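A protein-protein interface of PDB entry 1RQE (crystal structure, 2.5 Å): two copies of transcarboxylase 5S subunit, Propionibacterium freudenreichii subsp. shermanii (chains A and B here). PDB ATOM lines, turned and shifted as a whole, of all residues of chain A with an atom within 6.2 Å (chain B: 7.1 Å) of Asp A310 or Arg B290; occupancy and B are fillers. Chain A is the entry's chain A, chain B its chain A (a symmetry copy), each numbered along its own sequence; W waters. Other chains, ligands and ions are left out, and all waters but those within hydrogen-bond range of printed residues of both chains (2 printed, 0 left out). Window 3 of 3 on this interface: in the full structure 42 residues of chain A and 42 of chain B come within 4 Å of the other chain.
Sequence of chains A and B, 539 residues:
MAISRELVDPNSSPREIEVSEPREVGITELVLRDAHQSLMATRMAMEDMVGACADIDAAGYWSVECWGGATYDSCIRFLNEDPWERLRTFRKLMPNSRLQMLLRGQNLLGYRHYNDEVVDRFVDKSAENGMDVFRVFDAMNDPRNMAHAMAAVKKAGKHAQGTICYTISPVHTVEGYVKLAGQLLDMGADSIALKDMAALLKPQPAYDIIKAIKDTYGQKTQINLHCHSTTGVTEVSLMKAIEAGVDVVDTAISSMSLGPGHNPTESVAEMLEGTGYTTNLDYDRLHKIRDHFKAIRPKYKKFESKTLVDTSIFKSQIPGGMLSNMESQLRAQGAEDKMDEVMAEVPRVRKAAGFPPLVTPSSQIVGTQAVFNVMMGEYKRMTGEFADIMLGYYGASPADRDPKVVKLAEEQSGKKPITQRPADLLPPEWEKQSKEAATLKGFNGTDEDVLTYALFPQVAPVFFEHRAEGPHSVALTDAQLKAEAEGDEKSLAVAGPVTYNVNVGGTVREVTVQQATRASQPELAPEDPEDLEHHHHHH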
ATOM      1  N   ALA A 198     -25.539  19.845 -39.797  1.00  0.00           N
ATOM      2  CA  ALA A 198     -25.322  18.813 -38.794  1.00  0.00           C
ATOM      3  C   ALA A 198     -24.037  18.960 -37.995  1.00  0.00           C
ATOM      4  O   ALA A 198     -23.739  18.116 -37.156  1.00  0.00           O
ATOM      5  CB  ALA A 198     -25.368  17.434 -39.461  1.00  0.00           C
ATOM      6  N   SER A 229     -23.342  23.971 -33.986  1.00  0.00           N
ATOM      7  CA  SER A 229     -22.416  23.532 -32.947  1.00  0.00           C
ATOM      8  C   SER A 229     -22.812  22.193 -32.329  1.00  0.00           C
ATOM      9  O   SER A 229     -22.349  21.840 -31.248  1.00  0.00           O
ATOM     10  CB  SER A 229     -22.383  24.579 -31.846  1.00  0.00           C
ATOM     11  OG  SER A 229     -23.688  24.753 -31.298  1.00  0.00           O
ATOM     12  N   THR A 230     -23.659  21.453 -33.024  1.00  0.00           N
ATOM     13  CA  THR A 230     -24.158  20.182 -32.525  1.00  0.00           C
ATOM     14  C   THR A 230     -23.096  19.199 -32.031  1.00  0.00           C
ATOM     15  O   THR A 230     -23.273  18.542 -31.010  1.00  0.00           O
ATOM     16  CB  THR A 230     -24.988  19.478 -33.607  1.00  0.00           C
ATOM     17  OG1 THR A 230     -25.775  20.445 -34.311  1.00  0.00           O
ATOM     18  CG2 THR A 230     -25.908  18.459 -32.978  1.00  0.00           C
ATOM     19  N   THR A 231     -21.994  19.111 -32.761  1.00  0.00           N
ATOM     20  CA  THR A 231     -20.911  18.188 -32.447  1.00  0.00           C
ATOM     21  C   THR A 231     -19.788  18.752 -31.561  1.00  0.00           C
ATOM     22  O   THR A 231     -18.901  18.014 -31.113  1.00  0.00           O
ATOM     23  CB  THR A 231     -20.289  17.690 -33.745  1.00  0.00           C
ATOM     24  OG1 THR A 231     -19.818  18.817 -34.494  1.00  0.00           O
ATOM     25  CG2 THR A 231     -21.316  16.941 -34.568  1.00  0.00           C
ATOM     26  N   GLY A 232     -19.810  20.061 -31.338  1.00  0.00           N
ATOM     27  CA  GLY A 232     -18.812  20.689 -30.497  1.00  0.00           C
ATOM     28  C   GLY A 232     -17.465  21.005 -31.109  1.00  0.00           C
ATOM     29  O   GLY A 232     -16.595  21.508 -30.400  1.00  0.00           O
ATOM     30  N   THR A 307     -29.786  18.196 -25.193  1.00  0.00           N
ATOM     31  CA  THR A 307     -28.398  17.801 -25.428  1.00  0.00           C
ATOM     32  C   THR A 307     -27.592  18.972 -25.966  1.00  0.00           C
ATOM     33  O   THR A 307     -28.047  19.689 -26.856  1.00  0.00           O
ATOM     34  CB  THR A 307     -28.280  16.635 -26.436  1.00  0.00           C
ATOM     35  OG1 THR A 307     -29.195  15.588 -26.082  1.00  0.00           O
ATOM     36  CG2 THR A 307     -26.852  16.074 -26.424  1.00  0.00           C
ATOM     37  N   LEU A 308     -26.394  19.147 -25.419  1.00  0.00           N
ATOM     38  CA  LEU A 308     -25.496  20.228 -25.800  1.00  0.00           C
ATOM     39  C   LEU A 308     -24.422  19.801 -26.779  1.00  0.00           C
ATOM     40  O   LEU A 308     -24.041  20.565 -27.668  1.00  0.00           O
ATOM     41  CB  LEU A 308     -24.786  20.810 -24.571  1.00  0.00           C
ATOM     42  CG  LEU A 308     -25.514  21.787 -23.654  1.00  0.00           C
ATOM     43  CD1 LEU A 308     -24.533  22.288 -22.610  1.00  0.00           C
ATOM     44  CD2 LEU A 308     -26.068  22.958 -24.454  1.00  0.00           C
ATOM     45  N   VAL A 309     -23.920  18.587 -26.602  1.00  0.00           N
ATOM     46  CA  VAL A 309     -22.854  18.094 -27.452  1.00  0.00           C
ATOM     47  C   VAL A 309     -23.060  16.640 -27.797  1.00  0.00           C
ATOM     48  O   VAL A 309     -23.246  15.801 -26.921  1.00  0.00           O
ATOM     49  CB  VAL A 309     -21.492  18.246 -26.746  1.00  0.00           C
ATOM     50  CG1 VAL A 309     -20.367  17.854 -27.682  1.00  0.00           C
ATOM     51  CG2 VAL A 309     -21.316  19.673 -26.283  1.00  0.00           C
ATOM     52  N   ASP A 310     -23.017  16.344 -29.087  1.00  0.00           N
ATOM     53  CA  ASP A 310     -23.189  14.982 -29.552  1.00  0.00           C
ATOM     54  C   ASP A 310     -22.291  14.746 -30.754  1.00  0.00           C
ATOM     55  O   ASP A 310     -22.466  15.376 -31.787  1.00  0.00           O
ATOM     56  CB  ASP A 310     -24.637  14.737 -29.931  1.00  0.00           C
ATOM     57  CG  ASP A 310     -24.927  13.279 -30.170  1.00  0.00           C
ATOM     58  OD1 ASP A 310     -23.965  12.469 -30.146  1.00  0.00           O
ATOM     59  OD2 ASP A 310     -26.112  12.947 -30.383  1.00  0.00           O
ATOM     60  N   THR A 311     -21.329  13.842 -30.603  1.00  0.00           N
ATOM     61  CA  THR A 311     -20.378  13.526 -31.656  1.00  0.00           C
ATOM     62  C   THR A 311     -20.725  12.205 -32.328  1.00  0.00           C
ATOM     63  O   THR A 311     -20.056  11.790 -33.279  1.00  0.00           O
ATOM     64  CB  THR A 311     -18.946  13.384 -31.096  1.00  0.00           C
ATOM     65  OG1 THR A 311     -18.902  12.281 -30.183  1.00  0.00           O
ATOM     66  CG2 THR A 311     -18.508  14.648 -30.374  1.00  0.00           C
ATOM     67  N   SER A 312     -21.765  11.544 -31.832  1.00  0.00           N
ATOM     68  CA  SER A 312     -22.170  10.254 -32.368  1.00  0.00           C
ATOM     69  C   SER A 312     -22.297  10.234 -33.893  1.00  0.00           C
ATOM     70  O   SER A 312     -21.911   9.255 -34.547  1.00  0.00           O
ATOM     71  CB  SER A 312     -23.489   9.824 -31.729  1.00  0.00           C
ATOM     72  OG  SER A 312     -24.519  10.751 -32.045  1.00  0.00           O
ATOM     73  N   ILE A 313     -22.828  11.312 -34.463  1.00  0.00           N
ATOM     74  CA  ILE A 313     -23.015  11.386 -35.904  1.00  0.00           C
ATOM     75  C   ILE A 313     -21.740  11.097 -36.696  1.00  0.00           C
ATOM     76  O   ILE A 313     -21.809  10.617 -37.829  1.00  0.00           O
ATOM     77  CB  ILE A 313     -23.565  12.770 -36.336  1.00  0.00           C
ATOM     78  CG1 ILE A 313     -23.959  12.732 -37.825  1.00  0.00           C
ATOM     79  CG2 ILE A 313     -22.514  13.852 -36.091  1.00  0.00           C
ATOM     80  CD1 ILE A 313     -24.749  13.935 -38.301  1.00  0.00           C
ATOM     81  N   PHE A 314     -20.575  11.388 -36.128  1.00  0.00           N
ATOM     82  CA  PHE A 314     -19.330  11.107 -36.855  1.00  0.00           C
ATOM     83  C   PHE A 314     -19.155   9.623 -37.145  1.00  0.00           C
ATOM     84  O   PHE A 314     -18.513   9.252 -38.125  1.00  0.00           O
ATOM     85  CB  PHE A 314     -18.114  11.632 -36.090  1.00  0.00           C
ATOM     86  CG  PHE A 314     -17.972  13.115 -36.154  1.00  0.00           C
ATOM     87  CD1 PHE A 314     -17.893  13.874 -34.992  1.00  0.00           C
ATOM     88  CD2 PHE A 314     -17.945  13.766 -37.384  1.00  0.00           C
ATOM     89  CE1 PHE A 314     -17.792  15.270 -35.050  1.00  0.00           C
ATOM     90  CE2 PHE A 314     -17.843  15.161 -37.454  1.00  0.00           C
ATOM     91  CZ  PHE A 314     -17.767  15.912 -36.281  1.00  0.00           C
ATOM     92  N   GLY A 320     -29.242  13.692 -34.926  1.00  0.00           N
ATOM     93  CA  GLY A 320     -30.186  13.447 -33.845  1.00  0.00           C
ATOM     94  C   GLY A 320     -31.643  13.667 -34.220  1.00  0.00           C
ATOM     95  O   GLY A 320     -32.486  12.811 -33.965  1.00  0.00           O
ATOM     96  N   LEU A 323     -32.592  10.803 -35.722  1.00  0.00           N
ATOM     97  CA  LEU A 323     -32.495   9.699 -34.787  1.00  0.00           C
ATOM     98  C   LEU A 323     -33.723   9.582 -33.891  1.00  0.00           C
ATOM     99  O   LEU A 323     -34.340   8.523 -33.814  1.00  0.00           O
ATOM    100  CB  LEU A 323     -31.253   9.874 -33.923  1.00  0.00           C
ATOM    101  CG  LEU A 323     -31.067   8.809 -32.850  1.00  0.00           C
ATOM    102  CD1 LEU A 323     -30.905   7.441 -33.505  1.00  0.00           C
ATOM    103  CD2 LEU A 323     -29.852   9.154 -32.007  1.00  0.00           C
ATOM    104  N   ALA B  52     -18.770   4.263 -13.787  1.00  0.00           N
ATOM    105  CA  ALA B  52     -18.100   4.681 -15.009  1.00  0.00           C
ATOM    106  C   ALA B  52     -16.595   4.443 -14.960  1.00  0.00           C
ATOM    107  O   ALA B  52     -15.910   4.550 -15.983  1.00  0.00           O
ATOM    108  CB  ALA B  52     -18.394   6.165 -15.289  1.00  0.00           C
ATOM    109  N   ILE B 253     -16.016  14.778 -20.369  1.00  0.00           N
ATOM    110  CA  ILE B 253     -16.839  13.933 -21.239  1.00  0.00           C
ATOM    111  C   ILE B 253     -18.041  14.779 -21.690  1.00  0.00           C
ATOM    112  O   ILE B 253     -18.617  15.513 -20.890  1.00  0.00           O
ATOM    113  CB  ILE B 253     -17.278  12.655 -20.480  1.00  0.00           C
ATOM    114  CG1 ILE B 253     -17.870  11.646 -21.459  1.00  0.00           C
ATOM    115  CG2 ILE B 253     -18.218  13.004 -19.340  1.00  0.00           C
ATOM    116  CD1 ILE B 253     -16.831  11.046 -22.366  1.00  0.00           C
ATOM    117  N   SER B 254     -18.406  14.691 -22.969  1.00  0.00           N
ATOM    118  CA  SER B 254     -19.484  15.518 -23.528  1.00  0.00           C
ATOM    119  C   SER B 254     -20.777  15.782 -22.738  1.00  0.00           C
ATOM    120  O   SER B 254     -21.287  16.898 -22.766  1.00  0.00           O
ATOM    121  CB  SER B 254     -19.847  15.026 -24.934  1.00  0.00           C
ATOM    122  OG  SER B 254     -20.323  13.695 -24.920  1.00  0.00           O
ATOM    123  N   SER B 255     -21.316  14.788 -22.039  1.00  0.00           N
ATOM    124  CA  SER B 255     -22.553  14.993 -21.280  1.00  0.00           C
ATOM    125  C   SER B 255     -22.340  15.781 -19.991  1.00  0.00           C
ATOM    126  O   SER B 255     -23.295  16.091 -19.277  1.00  0.00           O
ATOM    127  CB  SER B 255     -23.207  13.650 -20.952  1.00  0.00           C
ATOM    128  OG  SER B 255     -22.255  12.739 -20.434  1.00  0.00           O
ATOM    129  N   MET B 256     -21.084  16.107 -19.699  1.00  0.00           N
ATOM    130  CA  MET B 256     -20.739  16.869 -18.507  1.00  0.00           C
ATOM    131  C   MET B 256     -19.806  18.004 -18.901  1.00  0.00           C
ATOM    132  O   MET B 256     -18.803  18.257 -18.230  1.00  0.00           O
ATOM    133  CB  MET B 256     -20.044  15.959 -17.503  1.00  0.00           C
ATOM    134  CG  MET B 256     -20.933  14.903 -16.906  1.00  0.00           C
ATOM    135  SD  MET B 256     -22.072  15.576 -15.677  1.00  0.00           S
ATOM    136  CE  MET B 256     -21.038  15.630 -14.215  1.00  0.00           C
ATOM    137  N   GLU B 266     -14.798  14.245 -26.296  1.00  0.00           N
ATOM    138  CA  GLU B 266     -15.097  13.731 -27.637  1.00  0.00           C
ATOM    139  C   GLU B 266     -14.868  14.760 -28.742  1.00  0.00           C
ATOM    140  O   GLU B 266     -14.295  14.442 -29.784  1.00  0.00           O
ATOM    141  CB  GLU B 266     -16.540  13.218 -27.706  1.00  0.00           C
ATOM    142  CG  GLU B 266     -16.818  12.029 -26.804  1.00  0.00           C
ATOM    143  CD  GLU B 266     -17.560  12.415 -25.548  1.00  0.00           C
ATOM    144  OE1 GLU B 266     -17.070  13.301 -24.809  1.00  0.00           O
ATOM    145  OE2 GLU B 266     -18.637  11.829 -25.301  1.00  0.00           O
ATOM    146  N   SER B 267     -15.323  15.988 -28.513  1.00  0.00           N
ATOM    147  CA  SER B 267     -15.152  17.066 -29.477  1.00  0.00           C
ATOM    148  C   SER B 267     -13.669  17.350 -29.755  1.00  0.00           C
ATOM    149  O   SER B 267     -13.256  17.489 -30.906  1.00  0.00           O
ATOM    150  CB  SER B 267     -15.829  18.330 -28.949  1.00  0.00           C
ATOM    151  OG  SER B 267     -17.231  18.162 -28.906  1.00  0.00           O
ATOM    152  N   ASP B 284     -15.550   4.076 -28.353  1.00  0.00           N
ATOM    153  CA  ASP B 284     -16.670   3.338 -27.796  1.00  0.00           C
ATOM    154  C   ASP B 284     -16.663   3.472 -26.275  1.00  0.00           C
ATOM    155  O   ASP B 284     -17.720   3.557 -25.658  1.00  0.00           O
ATOM    156  CB  ASP B 284     -16.625   1.865 -28.204  1.00  0.00           C
ATOM    157  CG  ASP B 284     -17.760   1.062 -27.583  1.00  0.00           C
ATOM    158  OD1 ASP B 284     -18.938   1.471 -27.726  1.00  0.00           O
ATOM    159  OD2 ASP B 284     -17.479   0.021 -26.943  1.00  0.00           O
ATOM    160  N   ARG B 285     -15.481   3.498 -25.666  1.00  0.00           N
ATOM    161  CA  ARG B 285     -15.398   3.667 -24.217  1.00  0.00           C
ATOM    162  C   ARG B 285     -15.908   5.058 -23.880  1.00  0.00           C
ATOM    163  O   ARG B 285     -16.699   5.235 -22.955  1.00  0.00           O
ATOM    164  CB  ARG B 285     -13.959   3.531 -23.725  1.00  0.00           C
ATOM    165  CG  ARG B 285     -13.405   2.120 -23.769  1.00  0.00           C
ATOM    166  CD  ARG B 285     -14.076   1.204 -22.747  1.00  0.00           C
ATOM    167  NE  ARG B 285     -13.429  -0.100 -22.746  1.00  0.00           N
ATOM    168  CZ  ARG B 285     -13.655  -1.072 -21.869  1.00  0.00           C
ATOM    169  NH1 ARG B 285     -14.533  -0.927 -20.884  1.00  0.00           N
ATOM    170  NH2 ARG B 285     -12.966  -2.195 -21.968  1.00  0.00           N
ATOM    171  N   LEU B 286     -15.446   6.051 -24.630  1.00  0.00           N
ATOM    172  CA  LEU B 286     -15.891   7.420 -24.398  1.00  0.00           C
ATOM    173  C   LEU B 286     -17.409   7.495 -24.467  1.00  0.00           C
ATOM    174  O   LEU B 286     -18.038   8.223 -23.702  1.00  0.00           O
ATOM    175  CB  LEU B 286     -15.307   8.366 -25.447  1.00  0.00           C
ATOM    176  CG  LEU B 286     -13.798   8.573 -25.432  1.00  0.00           C
ATOM    177  CD1 LEU B 286     -13.443   9.626 -26.454  1.00  0.00           C
ATOM    178  CD2 LEU B 286     -13.345   8.994 -24.038  1.00  0.00           C
ATOM    179  N   HIS B 287     -17.993   6.733 -25.386  1.00  0.00           N
ATOM    180  CA  HIS B 287     -19.436   6.722 -25.561  1.00  0.00           C
ATOM    181  C   HIS B 287     -20.191   6.175 -24.348  1.00  0.00           C
ATOM    182  O   HIS B 287     -21.296   6.623 -24.033  1.00  0.00           O
ATOM    183  CB  HIS B 287     -19.797   5.898 -26.786  1.00  0.00           C
ATOM    184  CG  HIS B 287     -21.250   5.939 -27.116  1.00  0.00           C
ATOM    185  ND1 HIS B 287     -21.837   7.016 -27.739  1.00  0.00           N
ATOM    186  CD2 HIS B 287     -22.249   5.066 -26.846  1.00  0.00           C
ATOM    187  CE1 HIS B 287     -23.137   6.806 -27.839  1.00  0.00           C
ATOM    188  NE2 HIS B 287     -23.413   5.631 -27.304  1.00  0.00           N
ATOM    189  N   LYS B 288     -19.605   5.197 -23.672  1.00  0.00           N
ATOM    190  CA  LYS B 288     -20.248   4.623 -22.494  1.00  0.00           C
ATOM    191  C   LYS B 288     -20.151   5.599 -21.330  1.00  0.00           C
ATOM    192  O   LYS B 288     -21.112   5.787 -20.578  1.00  0.00           O
ATOM    193  CB  LYS B 288     -19.593   3.291 -22.107  1.00  0.00           C
ATOM    194  CG  LYS B 288     -19.700   2.218 -23.166  1.00  0.00           C
ATOM    195  CD  LYS B 288     -18.962   0.990 -22.713  1.00  0.00           C
ATOM    196  CE  LYS B 288     -18.883  -0.060 -23.795  1.00  0.00           C
ATOM    197  NZ  LYS B 288     -18.071  -1.224 -23.302  1.00  0.00           N
ATOM    198  N   ILE B 289     -18.980   6.211 -21.184  1.00  0.00           N
ATOM    199  CA  ILE B 289     -18.749   7.179 -20.126  1.00  0.00           C
ATOM    200  C   ILE B 289     -19.772   8.301 -20.305  1.00  0.00           C
ATOM    201  O   ILE B 289     -20.409   8.757 -19.352  1.00  0.00           O
ATOM    202  CB  ILE B 289     -17.334   7.771 -20.233  1.00  0.00           C
ATOM    203  CG1 ILE B 289     -16.302   6.647 -20.152  1.00  0.00           C
ATOM    204  CG2 ILE B 289     -17.092   8.762 -19.123  1.00  0.00           C
ATOM    205  CD1 ILE B 289     -14.882   7.125 -20.367  1.00  0.00           C
ATOM    206  N   ARG B 290     -19.927   8.730 -21.550  1.00  0.00           N
ATOM    207  CA  ARG B 290     -20.848   9.798 -21.882  1.00  0.00           C
ATOM    208  C   ARG B 290     -22.298   9.459 -21.541  1.00  0.00           C
ATOM    209  O   ARG B 290     -22.993  10.254 -20.902  1.00  0.00           O
ATOM    210  CB  ARG B 290     -20.720  10.123 -23.358  1.00  0.00           C
ATOM    211  CG  ARG B 290     -21.728  11.096 -23.827  1.00  0.00           C
ATOM    212  CD  ARG B 290     -22.193  10.691 -25.175  1.00  0.00           C
ATOM    213  NE  ARG B 290     -23.369  11.455 -25.533  1.00  0.00           N
ATOM    214  CZ  ARG B 290     -24.156  11.164 -26.559  1.00  0.00           C
ATOM    215  NH1 ARG B 290     -23.879  10.113 -27.331  1.00  0.00           N
ATOM    216  NH2 ARG B 290     -25.223  11.925 -26.803  1.00  0.00           N
ATOM    217  N   ASP B 291     -22.756   8.284 -21.959  1.00  0.00           N
ATOM    218  CA  ASP B 291     -24.127   7.877 -21.679  1.00  0.00           C
ATOM    219  C   ASP B 291     -24.342   7.700 -20.189  1.00  0.00           C
ATOM    220  O   ASP B 291     -25.386   8.071 -19.645  1.00  0.00           O
ATOM    221  CB  ASP B 291     -24.466   6.565 -22.394  1.00  0.00           C
ATOM    222  CG  ASP B 291     -24.739   6.759 -23.881  1.00  0.00           C
ATOM    223  OD1 ASP B 291     -24.904   7.925 -24.314  1.00  0.00           O
ATOM    224  OD2 ASP B 291     -24.801   5.740 -24.611  1.00  0.00           O
ATOM    225  N   HIS B 292     -23.351   7.127 -19.527  1.00  0.00           N
ATOM    226  CA  HIS B 292     -23.458   6.922 -18.104  1.00  0.00           C
ATOM    227  C   HIS B 292     -23.852   8.239 -17.454  1.00  0.00           C
ATOM    228  O   HIS B 292     -24.808   8.298 -16.691  1.00  0.00           O
ATOM    229  CB  HIS B 292     -22.127   6.456 -17.528  1.00  0.00           C
ATOM    230  CG  HIS B 292     -22.107   6.437 -16.036  1.00  0.00           C
ATOM    231  ND1 HIS B 292     -22.577   5.371 -15.299  1.00  0.00           N
ATOM    232  CD2 HIS B 292     -21.773   7.396 -15.140  1.00  0.00           C
ATOM    233  CE1 HIS B 292     -22.537   5.674 -14.014  1.00  0.00           C
ATOM    234  NE2 HIS B 292     -22.054   6.897 -13.890  1.00  0.00           N
ATOM    235  N   PHE B 293     -23.116   9.304 -17.760  1.00  0.00           N
ATOM    236  CA  PHE B 293     -23.411  10.594 -17.152  1.00  0.00           C
ATOM    237  C   PHE B 293     -24.618  11.336 -17.699  1.00  0.00           C
ATOM    238  O   PHE B 293     -25.203  12.163 -17.008  1.00  0.00           O
ATOM    239  CB  PHE B 293     -22.170  11.474 -17.167  1.00  0.00           C
ATOM    240  CG  PHE B 293     -21.120  11.033 -16.177  1.00  0.00           C
ATOM    241  CD1 PHE B 293     -19.988  10.338 -16.596  1.00  0.00           C
ATOM    242  CD2 PHE B 293     -21.276  11.300 -14.815  1.00  0.00           C
ATOM    243  CE1 PHE B 293     -19.020   9.917 -15.675  1.00  0.00           C
ATOM    244  CE2 PHE B 293     -20.319  10.883 -13.880  1.00  0.00           C
ATOM    245  CZ  PHE B 293     -19.189  10.194 -14.310  1.00  0.00           C
ATOM    246  N   LYS B 294     -25.015  11.038 -18.926  1.00  0.00           N
ATOM    247  CA  LYS B 294     -26.193  11.687 -19.478  1.00  0.00           C
ATOM    248  C   LYS B 294     -27.428  11.221 -18.689  1.00  0.00           C
ATOM    249  O   LYS B 294     -28.386  11.967 -18.496  1.00  0.00           O
ATOM    250  CB  LYS B 294     -26.346  11.331 -20.954  1.00  0.00           C
ATOM    251  CG  LYS B 294     -27.526  12.009 -21.613  1.00  0.00           C
ATOM    252  CD  LYS B 294     -27.444  11.948 -23.132  1.00  0.00           C
ATOM    253  CE  LYS B 294     -28.551  12.792 -23.752  1.00  0.00           C
ATOM    254  NZ  LYS B 294     -28.571  14.198 -23.221  1.00  0.00           N
ATOM    255  N   ALA B 295     -27.386   9.986 -18.219  1.00  0.00           N
ATOM    256  CA  ALA B 295     -28.496   9.426 -17.465  1.00  0.00           C
ATOM    257  C   ALA B 295     -28.532   9.990 -16.058  1.00  0.00           C
ATOM    258  O   ALA B 295     -29.593  10.292 -15.511  1.00  0.00           O
ATOM    259  CB  ALA B 295     -28.363   7.911 -17.398  1.00  0.00           C
ATOM    260  N   ILE B 296     -27.352  10.126 -15.475  1.00  0.00           N
ATOM    261  CA  ILE B 296     -27.224  10.622 -14.124  1.00  0.00           C
ATOM    262  C   ILE B 296     -27.389  12.134 -13.948  1.00  0.00           C
ATOM    263  O   ILE B 296     -28.047  12.588 -13.017  1.00  0.00           O
ATOM    264  CB  ILE B 296     -25.852  10.162 -13.555  1.00  0.00           C
ATOM    265  CG1 ILE B 296     -26.009   8.777 -12.934  1.00  0.00           C
ATOM    266  CG2 ILE B 296     -25.289  11.181 -12.576  1.00  0.00           C
ATOM    267  CD1 ILE B 296     -24.710   8.164 -12.494  1.00  0.00           C
HETATM  268  O   HOH W   1     -20.932  12.794 -27.847  1.00  0.00           O
HETATM  269  O   HOH W   2     -23.863  17.299 -23.986  1.00  0.00           O
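O of Thr A230 lies within hydrogen-bond range of N of Asp A310, at 2.9 Å. The side-chain carboxylate of Asp A310 sits at hydrogen-bond distance from the side-chain hydroxyl of Ser A312, at 2.6 Å. The side-chain hydroxyl of Ser B254 is in hydrogen-bond range of the side-chain carboxylate of Glu B266 (2.5 Å). OG of Ser B255 sits at hydrogen-bond distance from O of Arg B290 (2.6 Å). NH1 of Arg B290 is in salt-bridge range of OD1 of Asp B291.
CA of Gly A232 touches OG of Ser B267, at 3.4 Å. Val A309 touches Ser B254. CG1 of Val A309 touches OG of Ser B267, 3.4 Å away. Thr A311 touches Glu B266 (OG1 to CB, 3.5 Å). Thr A311 touches Ser B267 (CG2 to N, 3.9 Å).
Hydrophobic or aromatic side chains of chain A that line the printed part of chain B: Val A309.
No position is printed for both chains. Of the 8 pairs that touch across the chains among the printed residues, none has its exchanged pair printed and touching as well.
OG of Ser B267 is in hydrogen-bond range of O of Thr A231, at 2.8 Å. The side-chain hydroxyl of Thr A307 is in hydrogen-bond range of the side-chain amino group of Lys B294 (3.2 Å). The side-chain carboxylate (OD1) of Asp A310 is in salt-bridge range of the guanidinium group (NH2) of Arg B290.
Water W2 lies within hydrogen-bond range of O of Ser B254 (2.9 Å), N of Val A309 (2.9 Å) and N of Leu A308 (3.4 Å). Water W1 bridges N of Thr A311 (3.0 Å) and OG of Ser B254 (3.1 Å).
Of the printed residues of chain B, Gly A232 touches Ser B267 (3.4 Å). Of the printed residues of chain B, Val A309 touches Ser B254 and Ser B267. Of chain B, only Arg B290 (3.6 Å) comes within 4 Å of Asp A310. Met B256 touches none of the printed residues of chain A. Of the printed residues of chain A, Glu B266 touches Thr A311. Printed residues of chain A within 4 Å of Ser B267: Thr A231, Gly A232, Val A309 and Thr A311. Leu B286 touches none of the printed residues of chain A. Arg B290 touches just one residue of chain A: Asp A310 (3.6 Å). The nearest printed residue of chain A that does not touch Lys B294 is Leu A308 (5.8 Å).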
